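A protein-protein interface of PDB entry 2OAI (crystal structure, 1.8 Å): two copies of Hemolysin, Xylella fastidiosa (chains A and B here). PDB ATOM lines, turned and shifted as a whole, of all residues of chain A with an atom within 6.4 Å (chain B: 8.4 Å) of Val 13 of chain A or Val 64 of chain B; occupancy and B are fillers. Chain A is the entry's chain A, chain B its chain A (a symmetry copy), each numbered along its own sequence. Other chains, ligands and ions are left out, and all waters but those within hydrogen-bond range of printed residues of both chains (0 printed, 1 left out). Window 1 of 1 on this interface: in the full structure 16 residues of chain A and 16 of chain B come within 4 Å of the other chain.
The guanidinium group of Arg 15 of chain A lies within salt-bridge range of the side-chain carboxylate of Glu 76 of chain B (2.8 Å).
O of Val 13 of chain A is in hydrogen-bond range of N of Leu 21 of chain A. OG of Ser 19 of chain A is in hydrogen-bond range of NH1 of Arg 15 of chain A (3.0 Å). The backbone NH (N) of Val 78 of chain B sits at hydrogen-bond distance from O of MLY 87 of chain B, at 2.9 Å. The backbone carbonyl oxygen (O) of Asp 79 of chain B is in hydrogen-bond range of N of MLY 87 of chain B (3.1 Å).
Among the printed residues, merely in contact across the chains: MLY 87 of chain A with Asp 79 of chain B (3.3 Å), Val 13 of chain A with Val 64 of chain B (3.4 Å), Leu 21 of chain A with Val 64 of chain B (3.4 Å), MLY 87 of chain A with Val 78 of chain B (3.5 Å) and Leu 21 of chain A with Val 78 of chain B (3.9 Å).
Printed residues of chain B within 4 Å of Val 13 of chain A: Val 64. Printed residues of chain B within 4 Å of Leu 21 of chain A: Val 64 (3.4 Å) and Val 78 (3.9 Å). Of the printed residues of chain B, MLY 87 of chain A touches Val 78 and Asp 79. Val 64 of chain B touches just these residues of chain A: Val 13 (3.4 Å) and Leu 21 (3.4 Å). The nearest residue of chain B that does not touch Val 13 of chain A is Gly 65 of chain B (4.9 Å).
Of the 11 printed residues of chain A, 4 touch a printed residue of chain B. Printed residues of chain A that touch a printed residue of chain B: Val 13, Arg 15, Leu 21 and MLY 87. Hydrophobic or aromatic side chains of chain A within 4 Å of the printed part of chain B: Val 13 and Leu 21. Among the printed residues, 6 pairs touch across the chains. Among the printed residues, Asp or Glu carboxylates within 4 Å of a Lys or Arg side-chain nitrogen of the other chain: Arg 15 of chain A with Glu 76 of chain B.
1 position is printed for both chains. Of the 6 pairs that touch across the chains among the printed residues, none has its exchanged pair printed and touching as well.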
ATOM      1  N   ALA A  10     -26.260 -27.747 -18.498  1.00  0.00           N
ATOM      2  CA  ALA A  10     -26.642 -28.662 -19.592  1.00  0.00           C
ATOM      3  C   ALA A  10     -25.428 -29.474 -20.055  1.00  0.00           C
ATOM      4  O   ALA A  10     -24.330 -28.907 -20.176  1.00  0.00           O
ATOM      5  CB  ALA A  10     -27.185 -27.852 -20.764  1.00  0.00           C
ATOM      6  N   LEU A  11     -25.607 -30.771 -20.320  1.00  0.00           N
ATOM      7  CA  LEU A  11     -24.484 -31.604 -20.730  1.00  0.00           C
ATOM      8  C   LEU A  11     -24.262 -31.525 -22.237  1.00  0.00           C
ATOM      9  O   LEU A  11     -23.181 -31.844 -22.718  1.00  0.00           O
ATOM     10  CB  LEU A  11     -24.698 -33.062 -20.333  1.00  0.00           C
ATOM     11  CG  LEU A  11     -23.931 -33.639 -19.109  1.00  0.00           C
ATOM     12  CD1 LEU A  11     -23.529 -32.624 -18.069  1.00  0.00           C
ATOM     13  CD2 LEU A  11     -24.643 -34.841 -18.496  1.00  0.00           C
ATOM     14  N   MET A  12     -25.302 -31.134 -22.964  1.00  0.00           N
ATOM     15  CA  MET A  12     -25.231 -31.107 -24.421  1.00  0.00           C
ATOM     16  C   MET A  12     -26.107 -30.003 -24.964  1.00  0.00           C
ATOM     17  O   MET A  12     -27.249 -29.844 -24.523  1.00  0.00           O
ATOM     18  CB  MET A  12     -25.744 -32.421 -24.960  1.00  0.00           C
ATOM     19  CG  MET A  12     -25.066 -32.787 -26.187  1.00  0.00           C
ATOM     20  SD  MET A  12     -26.019 -34.300 -26.853  1.00  0.00           S
ATOM     21  CE  MET A  12     -27.204 -33.255 -28.015  1.00  0.00           C
ATOM     22  N   VAL A  13     -25.584 -29.224 -25.904  1.00  0.00           N
ATOM     23  CA  VAL A  13     -26.387 -28.183 -26.515  1.00  0.00           C
ATOM     24  C   VAL A  13     -26.154 -28.180 -28.019  1.00  0.00           C
ATOM     25  O   VAL A  13     -25.094 -28.582 -28.480  1.00  0.00           O
ATOM     26  CB  VAL A  13     -26.098 -26.756 -25.961  1.00  0.00           C
ATOM     27  CG1 VAL A  13     -26.133 -26.716 -24.383  1.00  0.00           C
ATOM     28  CG2 VAL A  13     -24.863 -26.235 -26.509  1.00  0.00           C
ATOM     29  N   THR A  14     -27.163 -27.743 -28.763  1.00  0.00           N
ATOM     30  CA  THR A  14     -27.095 -27.723 -30.215  1.00  0.00           C
ATOM     31  C   THR A  14     -26.745 -26.314 -30.663  1.00  0.00           C
ATOM     32  O   THR A  14     -27.407 -25.357 -30.252  1.00  0.00           O
ATOM     33  CB  THR A  14     -28.483 -28.062 -30.807  1.00  0.00           C
ATOM     34  OG1 THR A  14     -28.958 -29.267 -30.187  1.00  0.00           O
ATOM     35  CG2 THR A  14     -28.348 -28.280 -32.316  1.00  0.00           C
ATOM     36  N   ARG A  15     -25.750 -26.191 -31.524  1.00  0.00           N
ATOM     37  CA  ARG A  15     -25.428 -24.922 -32.174  1.00  0.00           C
ATOM     38  C   ARG A  15     -26.328 -24.611 -33.354  1.00  0.00           C
ATOM     39  O   ARG A  15     -27.062 -25.485 -33.866  1.00  0.00           O
ATOM     40  CB  ARG A  15     -23.958 -24.964 -32.639  1.00  0.00           C
ATOM     41  CG  ARG A  15     -22.963 -25.126 -31.471  1.00  0.00           C
ATOM     42  CD  ARG A  15     -21.556 -25.201 -32.051  1.00  0.00           C
ATOM     43  NE  ARG A  15     -21.142 -23.935 -32.660  1.00  0.00           N
ATOM     44  CZ  ARG A  15     -20.411 -23.827 -33.779  1.00  0.00           C
ATOM     45  NH1 ARG A  15     -20.085 -24.902 -34.504  1.00  0.00           N
ATOM     46  NH2 ARG A  15     -20.056 -22.627 -34.220  1.00  0.00           N
ATOM     47  N   SER A  19     -24.435 -28.593 -35.218  1.00  0.00           N
ATOM     48  CA  SER A  19     -23.337 -29.268 -34.498  1.00  0.00           C
ATOM     49  C   SER A  19     -23.628 -29.240 -32.991  1.00  0.00           C
ATOM     50  O   SER A  19     -24.532 -28.535 -32.550  1.00  0.00           O
ATOM     51  CB  SER A  19     -21.952 -28.646 -34.838  1.00  0.00           C
ATOM     52  OG  SER A  19     -21.903 -27.257 -34.536  1.00  0.00           O
ATOM     53  N   PHE A  20     -22.888 -30.040 -32.211  1.00  0.00           N
ATOM     54  CA  PHE A  20     -23.207 -30.182 -30.797  1.00  0.00           C
ATOM     55  C   PHE A  20     -22.019 -29.765 -29.987  1.00  0.00           C
ATOM     56  O   PHE A  20     -20.878 -30.143 -30.296  1.00  0.00           O
ATOM     57  CB  PHE A  20     -23.491 -31.651 -30.443  1.00  0.00           C
ATOM     58  CG  PHE A  20     -24.722 -32.243 -31.120  1.00  0.00           C
ATOM     59  CD1 PHE A  20     -25.940 -31.581 -31.102  1.00  0.00           C
ATOM     60  CD2 PHE A  20     -24.653 -33.489 -31.723  1.00  0.00           C
ATOM     61  CE1 PHE A  20     -27.072 -32.153 -31.715  1.00  0.00           C
ATOM     62  CE2 PHE A  20     -25.781 -34.077 -32.329  1.00  0.00           C
ATOM     63  CZ  PHE A  20     -26.978 -33.411 -32.333  1.00  0.00           C
ATOM     64  N   LEU A  21     -22.281 -29.052 -28.911  1.00  0.00           N
ATOM     65  CA  LEU A  21     -21.273 -28.801 -27.893  1.00  0.00           C
ATOM     66  C   LEU A  21     -21.609 -29.682 -26.683  1.00  0.00           C
ATOM     67  O   LEU A  21     -22.735 -29.622 -26.131  1.00  0.00           O
ATOM     68  CB  LEU A  21     -21.261 -27.324 -27.519  1.00  0.00           C
ATOM     69  CG  LEU A  21     -20.617 -26.440 -28.612  1.00  0.00           C
ATOM     70  CD1 LEU A  21     -20.985 -24.938 -28.426  1.00  0.00           C
ATOM     71  CD2 LEU A  21     -19.071 -26.605 -28.529  1.00  0.00           C
ATOM     72  N   ILE A  22     -20.634 -30.512 -26.286  1.00  0.00           N
ATOM     73  CA  ILE A  22     -20.906 -31.609 -25.341  1.00  0.00           C
ATOM     74  C   ILE A  22     -19.903 -31.618 -24.178  1.00  0.00           C
ATOM     75  O   ILE A  22     -18.707 -31.430 -24.376  1.00  0.00           O
ATOM     76  CB  ILE A  22     -20.887 -32.970 -26.044  1.00  0.00           C
ATOM     77  CG1 ILE A  22     -21.861 -32.961 -27.252  1.00  0.00           C
ATOM     78  CG2 ILE A  22     -21.256 -34.099 -25.026  1.00  0.00           C
ATOM     79  CD1 ILE A  22     -22.024 -34.329 -27.943  1.00  0.00           C
ATOM     80  N   MLY A  87     -15.110 -29.348 -22.612  1.00  0.00           N
ATOM     81  CA  MLY A  87     -16.126 -29.179 -23.650  1.00  0.00           C
ATOM     82  CB  MLY A  87     -16.543 -27.704 -23.743  1.00  0.00           C
ATOM     83  CG  MLY A  87     -17.937 -27.514 -24.383  1.00  0.00           C
ATOM     84  CD  MLY A  87     -19.013 -27.655 -23.255  1.00  0.00           C
ATOM     85  CE  MLY A  87     -20.426 -27.477 -23.748  1.00  0.00           C
ATOM     86  NZ  MLY A  87     -21.403 -27.348 -22.651  1.00  0.00           N
ATOM     87  CH1 MLY A  87     -22.698 -27.290 -23.340  1.00  0.00           C
ATOM     88  CH2 MLY A  87     -21.386 -28.553 -21.771  1.00  0.00           C
ATOM     89  C   MLY A  87     -15.574 -29.656 -24.969  1.00  0.00           C
ATOM     90  O   MLY A  87     -14.400 -29.364 -25.295  1.00  0.00           O
ATOM     91  N   ARG B  60     -27.843 -10.728 -19.214  1.00  0.00           N
ATOM     92  CA  ARG B  60     -28.086 -11.980 -18.488  1.00  0.00           C
ATOM     93  C   ARG B  60     -26.918 -12.908 -18.821  1.00  0.00           C
ATOM     94  O   ARG B  60     -26.087 -12.585 -19.675  1.00  0.00           O
ATOM     95  CB  ARG B  60     -29.412 -12.649 -18.922  1.00  0.00           C
ATOM     96  CG  ARG B  60     -29.531 -12.815 -20.427  1.00  0.00           C
ATOM     97  CD  ARG B  60     -30.871 -13.395 -20.905  1.00  0.00           C
ATOM     98  NE  ARG B  60     -30.928 -13.270 -22.359  1.00  0.00           N
ATOM     99  CZ  ARG B  60     -30.392 -14.142 -23.215  1.00  0.00           C
ATOM    100  NH1 ARG B  60     -30.465 -13.912 -24.511  1.00  0.00           N
ATOM    101  NH2 ARG B  60     -29.809 -15.252 -22.783  1.00  0.00           N
ATOM    102  N   ILE B  61     -26.847 -14.045 -18.142  1.00  0.00           N
ATOM    103  CA  ILE B  61     -25.863 -15.068 -18.474  1.00  0.00           C
ATOM    104  C   ILE B  61     -26.377 -15.843 -19.691  1.00  0.00           C
ATOM    105  O   ILE B  61     -27.370 -16.557 -19.595  1.00  0.00           O
ATOM    106  CB  ILE B  61     -25.617 -16.046 -17.311  1.00  0.00           C
ATOM    107  CG1 ILE B  61     -25.219 -15.274 -16.040  1.00  0.00           C
ATOM    108  CG2 ILE B  61     -24.520 -17.052 -17.715  1.00  0.00           C
ATOM    109  CD1 ILE B  61     -25.403 -16.050 -14.742  1.00  0.00           C
ATOM    110  N   PRO B  62     -25.676 -15.726 -20.828  1.00  0.00           N
ATOM    111  CA  PRO B  62     -26.172 -16.333 -22.085  1.00  0.00           C
ATOM    112  C   PRO B  62     -26.115 -17.864 -22.076  1.00  0.00           C
ATOM    113  O   PRO B  62     -25.396 -18.442 -21.259  1.00  0.00           O
ATOM    114  CB  PRO B  62     -25.241 -15.750 -23.146  1.00  0.00           C
ATOM    115  CG  PRO B  62     -23.942 -15.541 -22.406  1.00  0.00           C
ATOM    116  CD  PRO B  62     -24.371 -15.061 -21.006  1.00  0.00           C
ATOM    117  N   HIS B  63     -26.905 -18.522 -22.929  1.00  0.00           N
ATOM    118  CA  HIS B  63     -26.814 -19.964 -23.072  1.00  0.00           C
ATOM    119  C   HIS B  63     -25.627 -20.241 -23.998  1.00  0.00           C
ATOM    120  O   HIS B  63     -25.303 -19.446 -24.900  1.00  0.00           O
ATOM    121  CB  HIS B  63     -28.042 -20.562 -23.795  1.00  0.00           C
ATOM    122  CG  HIS B  63     -29.270 -20.684 -22.958  1.00  0.00           C
ATOM    123  ND1 HIS B  63     -29.853 -19.613 -22.312  1.00  0.00           N
ATOM    124  CD2 HIS B  63     -30.073 -21.752 -22.721  1.00  0.00           C
ATOM    125  CE1 HIS B  63     -30.941 -20.023 -21.681  1.00  0.00           C
ATOM    126  NE2 HIS B  63     -31.104 -21.316 -21.918  1.00  0.00           N
ATOM    127  N   VAL B  64     -25.009 -21.404 -23.836  1.00  0.00           N
ATOM    128  CA  VAL B  64     -24.041 -21.861 -24.847  1.00  0.00           C
ATOM    129  C   VAL B  64     -24.749 -21.904 -26.200  1.00  0.00           C
ATOM    130  O   VAL B  64     -25.898 -22.357 -26.291  1.00  0.00           O
ATOM    131  CB  VAL B  64     -23.459 -23.261 -24.485  1.00  0.00           C
ATOM    132  CG1 VAL B  64     -22.648 -23.840 -25.640  1.00  0.00           C
ATOM    133  CG2 VAL B  64     -22.608 -23.168 -23.190  1.00  0.00           C
ATOM    134  N   GLY B  65     -24.061 -21.415 -27.227  1.00  0.00           N
ATOM    135  CA  GLY B  65     -24.579 -21.379 -28.582  1.00  0.00           C
ATOM    136  C   GLY B  65     -25.167 -20.023 -28.970  1.00  0.00           C
ATOM    137  O   GLY B  65     -25.423 -19.786 -30.160  1.00  0.00           O
ATOM    138  N   GLU B  66     -25.430 -19.162 -27.996  1.00  0.00           N
ATOM    139  CA  GLU B  66     -25.863 -17.798 -28.326  1.00  0.00           C
ATOM    140  C   GLU B  66     -24.662 -17.011 -28.844  1.00  0.00           C
ATOM    141  O   GLU B  66     -23.521 -17.375 -28.559  1.00  0.00           O
ATOM    142  CB  GLU B  66     -26.500 -17.094 -27.144  1.00  0.00           C
ATOM    143  CG  GLU B  66     -27.829 -17.711 -26.709  1.00  0.00           C
ATOM    144  CD  GLU B  66     -28.559 -16.807 -25.733  1.00  0.00           C
ATOM    145  OE1 GLU B  66     -29.213 -15.843 -26.174  1.00  0.00           O
ATOM    146  OE2 GLU B  66     -28.475 -17.043 -24.509  1.00  0.00           O
ATOM    147  N   TYR B  67     -24.919 -15.996 -29.669  1.00  0.00           N
ATOM    148  CA  TYR B  67     -23.820 -15.232 -30.272  1.00  0.00           C
ATOM    149  C   TYR B  67     -24.256 -13.822 -30.586  1.00  0.00           C
ATOM    150  O   TYR B  67     -25.470 -13.513 -30.574  1.00  0.00           O
ATOM    151  CB  TYR B  67     -23.306 -15.890 -31.562  1.00  0.00           C
ATOM    152  CG  TYR B  67     -24.354 -15.977 -32.668  1.00  0.00           C
ATOM    153  CD1 TYR B  67     -24.549 -14.916 -33.575  1.00  0.00           C
ATOM    154  CD2 TYR B  67     -25.194 -17.096 -32.769  1.00  0.00           C
ATOM    155  CE1 TYR B  67     -25.499 -15.009 -34.589  1.00  0.00           C
ATOM    156  CE2 TYR B  67     -26.148 -17.197 -33.771  1.00  0.00           C
ATOM    157  CZ  TYR B  67     -26.295 -16.146 -34.680  1.00  0.00           C
ATOM    158  OH  TYR B  67     -27.242 -16.239 -35.671  1.00  0.00           O
ATOM    159  N   GLU B  76     -19.326 -16.257 -30.090  1.00  0.00           N
ATOM    160  CA  GLU B  76     -20.290 -17.296 -29.730  1.00  0.00           C
ATOM    161  C   GLU B  76     -19.890 -17.918 -28.397  1.00  0.00           C
ATOM    162  O   GLU B  76     -18.716 -18.205 -28.178  1.00  0.00           O
ATOM    163  CB  GLU B  76     -20.352 -18.359 -30.841  1.00  0.00           C
ATOM    164  CG  GLU B  76     -21.284 -19.527 -30.449  1.00  0.00           C
ATOM    165  CD  GLU B  76     -21.395 -20.599 -31.545  1.00  0.00           C
ATOM    166  OE1 GLU B  76     -20.785 -20.435 -32.649  1.00  0.00           O
ATOM    167  OE2 GLU B  76     -22.086 -21.606 -31.279  1.00  0.00           O
ATOM    168  N   ILE B  77     -20.854 -18.099 -27.493  1.00  0.00           N
ATOM    169  CA  ILE B  77     -20.568 -18.705 -26.203  1.00  0.00           C
ATOM    170  C   ILE B  77     -20.377 -20.191 -26.455  1.00  0.00           C
ATOM    171  O   ILE B  77     -21.263 -20.826 -27.003  1.00  0.00           O
ATOM    172  CB  ILE B  77     -21.787 -18.537 -25.240  1.00  0.00           C
ATOM    173  CG1 ILE B  77     -22.170 -17.043 -25.138  1.00  0.00           C
ATOM    174  CG2 ILE B  77     -21.511 -19.240 -23.870  1.00  0.00           C
ATOM    175  CD1 ILE B  77     -21.092 -16.189 -24.722  1.00  0.00           C
ATOM    176  N   VAL B  78     -19.242 -20.764 -26.059  1.00  0.00           N
ATOM    177  CA  VAL B  78     -19.106 -22.220 -26.289  1.00  0.00           C
ATOM    178  C   VAL B  78     -18.947 -23.061 -25.026  1.00  0.00           C
ATOM    179  O   VAL B  78     -19.167 -24.269 -25.076  1.00  0.00           O
ATOM    180  CB  VAL B  78     -18.048 -22.602 -27.343  1.00  0.00           C
ATOM    181  CG1 VAL B  78     -18.403 -22.037 -28.750  1.00  0.00           C
ATOM    182  CG2 VAL B  78     -16.711 -22.221 -26.877  1.00  0.00           C
ATOM    183  N   ASP B  79     -18.623 -22.419 -23.896  1.00  0.00           N
ATOM    184  CA  ASP B  79     -18.628 -23.118 -22.607  1.00  0.00           C
ATOM    185  C   ASP B  79     -18.925 -22.218 -21.457  1.00  0.00           C
ATOM    186  O   ASP B  79     -18.344 -21.147 -21.370  1.00  0.00           O
ATOM    187  CB  ASP B  79     -17.288 -23.797 -22.316  1.00  0.00           C
ATOM    188  CG  ASP B  79     -17.314 -24.575 -21.004  1.00  0.00           C
ATOM    189  OD1 ASP B  79     -18.140 -25.497 -20.872  1.00  0.00           O
ATOM    190  OD2 ASP B  79     -16.535 -24.261 -20.101  1.00  0.00           O
ATOM    191  N   LEU B  80     -19.814 -22.697 -20.574  1.00  0.00           N
ATOM    192  CA  LEU B  80     -20.051 -22.068 -19.266  1.00  0.00           C
ATOM    193  C   LEU B  80     -19.497 -22.989 -18.189  1.00  0.00           C
ATOM    194  O   LEU B  80     -19.511 -24.230 -18.348  1.00  0.00           O
ATOM    195  CB  LEU B  80     -21.558 -21.895 -19.043  1.00  0.00           C
ATOM    196  CG  LEU B  80     -22.329 -21.003 -20.031  1.00  0.00           C
ATOM    197  CD1 LEU B  80     -23.820 -21.047 -19.704  1.00  0.00           C
ATOM    198  CD2 LEU B  80     -21.820 -19.569 -19.960  1.00  0.00           C
ATOM    199  N   ASP B  81     -19.052 -22.403 -17.082  1.00  0.00           N
ATOM    200  CA  ASP B  81     -18.831 -23.186 -15.872  1.00  0.00           C
ATOM    201  C   ASP B  81     -19.690 -22.543 -14.828  1.00  0.00           C
ATOM    202  O   ASP B  81     -19.297 -21.508 -14.269  1.00  0.00           O
ATOM    203  CB  ASP B  81     -17.364 -23.189 -15.471  1.00  0.00           C
ATOM    204  CG  ASP B  81     -16.503 -23.843 -16.508  1.00  0.00           C
ATOM    205  OD1 ASP B  81     -16.954 -24.837 -17.117  1.00  0.00           O
ATOM    206  OD2 ASP B  81     -15.391 -23.382 -16.736  1.00  0.00           O
ATOM    207  N   GLY B  82     -20.881 -23.102 -14.632  1.00  0.00           N
ATOM    208  CA  GLY B  82     -21.868 -22.444 -13.766  1.00  0.00           C
ATOM    209  C   GLY B  82     -22.178 -21.100 -14.398  1.00  0.00           C
ATOM    210  O   GLY B  82     -22.532 -21.032 -15.567  1.00  0.00           O
ATOM    211  N   ARG B  84     -19.966 -18.689 -14.939  1.00  0.00           N
ATOM    212  CA  ARG B  84     -18.799 -18.156 -15.641  1.00  0.00           C
ATOM    213  C   ARG B  84     -18.888 -18.432 -17.135  1.00  0.00           C
ATOM    214  O   ARG B  84     -19.113 -19.570 -17.550  1.00  0.00           O
ATOM    215  CB  ARG B  84     -17.495 -18.733 -15.071  1.00  0.00           C
ATOM    216  CG  ARG B  84     -16.221 -18.167 -15.726  1.00  0.00           C
ATOM    217  CD  ARG B  84     -14.949 -18.665 -15.024  1.00  0.00           C
ATOM    218  NE  ARG B  84     -14.704 -20.093 -15.274  1.00  0.00           N
ATOM    219  CZ  ARG B  84     -14.022 -20.898 -14.456  1.00  0.00           C
ATOM    220  NH1 ARG B  84     -13.520 -20.433 -13.310  1.00  0.00           N
ATOM    221  NH2 ARG B  84     -13.857 -22.182 -14.766  1.00  0.00           N
ATOM    222  N   ILE B  85     -18.721 -17.385 -17.938  1.00  0.00           N
ATOM    223  CA  ILE B  85     -18.594 -17.556 -19.404  1.00  0.00           C
ATOM    224  C   ILE B  85     -17.137 -17.937 -19.629  1.00  0.00           C
ATOM    225  O   ILE B  85     -16.230 -17.071 -19.645  1.00  0.00           O
ATOM    226  CB  ILE B  85     -18.971 -16.281 -20.171  1.00  0.00           C
ATOM    227  CG1 ILE B  85     -20.404 -15.865 -19.800  1.00  0.00           C
ATOM    228  CG2 ILE B  85     -18.744 -16.470 -21.698  1.00  0.00           C
ATOM    229  CD1 ILE B  85     -20.848 -14.554 -20.403  1.00  0.00           C
ATOM    230  N   ASP B  86     -16.916 -19.233 -19.801  1.00  0.00           N
ATOM    231  CA  ASP B  86     -15.577 -19.752 -19.731  1.00  0.00           C
ATOM    232  C   ASP B  86     -14.830 -19.767 -21.072  1.00  0.00           C
ATOM    233  O   ASP B  86     -13.632 -19.517 -21.086  1.00  0.00           O
ATOM    234  CB  ASP B  86     -15.550 -21.122 -19.069  1.00  0.00           C
ATOM    235  CG  ASP B  86     -14.136 -21.557 -18.695  1.00  0.00           C
ATOM    236  OD1 ASP B  86     -13.481 -20.816 -17.919  1.00  0.00           O
ATOM    237  OD2 ASP B  86     -13.644 -22.620 -19.201  1.00  0.00           O
ATOM    238  N   MLY B  87     -15.526 -20.030 -22.183  1.00  0.00           N
ATOM    239  CA  MLY B  87     -14.857 -20.107 -23.481  1.00  0.00           C
ATOM    240  CB  MLY B  87     -14.501 -21.566 -23.804  1.00  0.00           C
ATOM    241  CG  MLY B  87     -13.354 -21.689 -24.832  1.00  0.00           C
ATOM    242  CD  MLY B  87     -11.996 -21.623 -24.058  1.00  0.00           C
ATOM    243  CE  MLY B  87     -10.789 -21.747 -24.951  1.00  0.00           C
ATOM    244  NZ  MLY B  87      -9.537 -21.948 -24.197  1.00  0.00           N
ATOM    245  CH1 MLY B  87      -8.498 -21.939 -25.234  1.00  0.00           C
ATOM    246  CH2 MLY B  87      -9.285 -20.815 -23.260  1.00  0.00           C
ATOM    247  C   MLY B  87     -15.761 -19.536 -24.542  1.00  0.00           C
ATOM    248  O   MLY B  87     -16.982 -19.815 -24.536  1.00  0.00           O
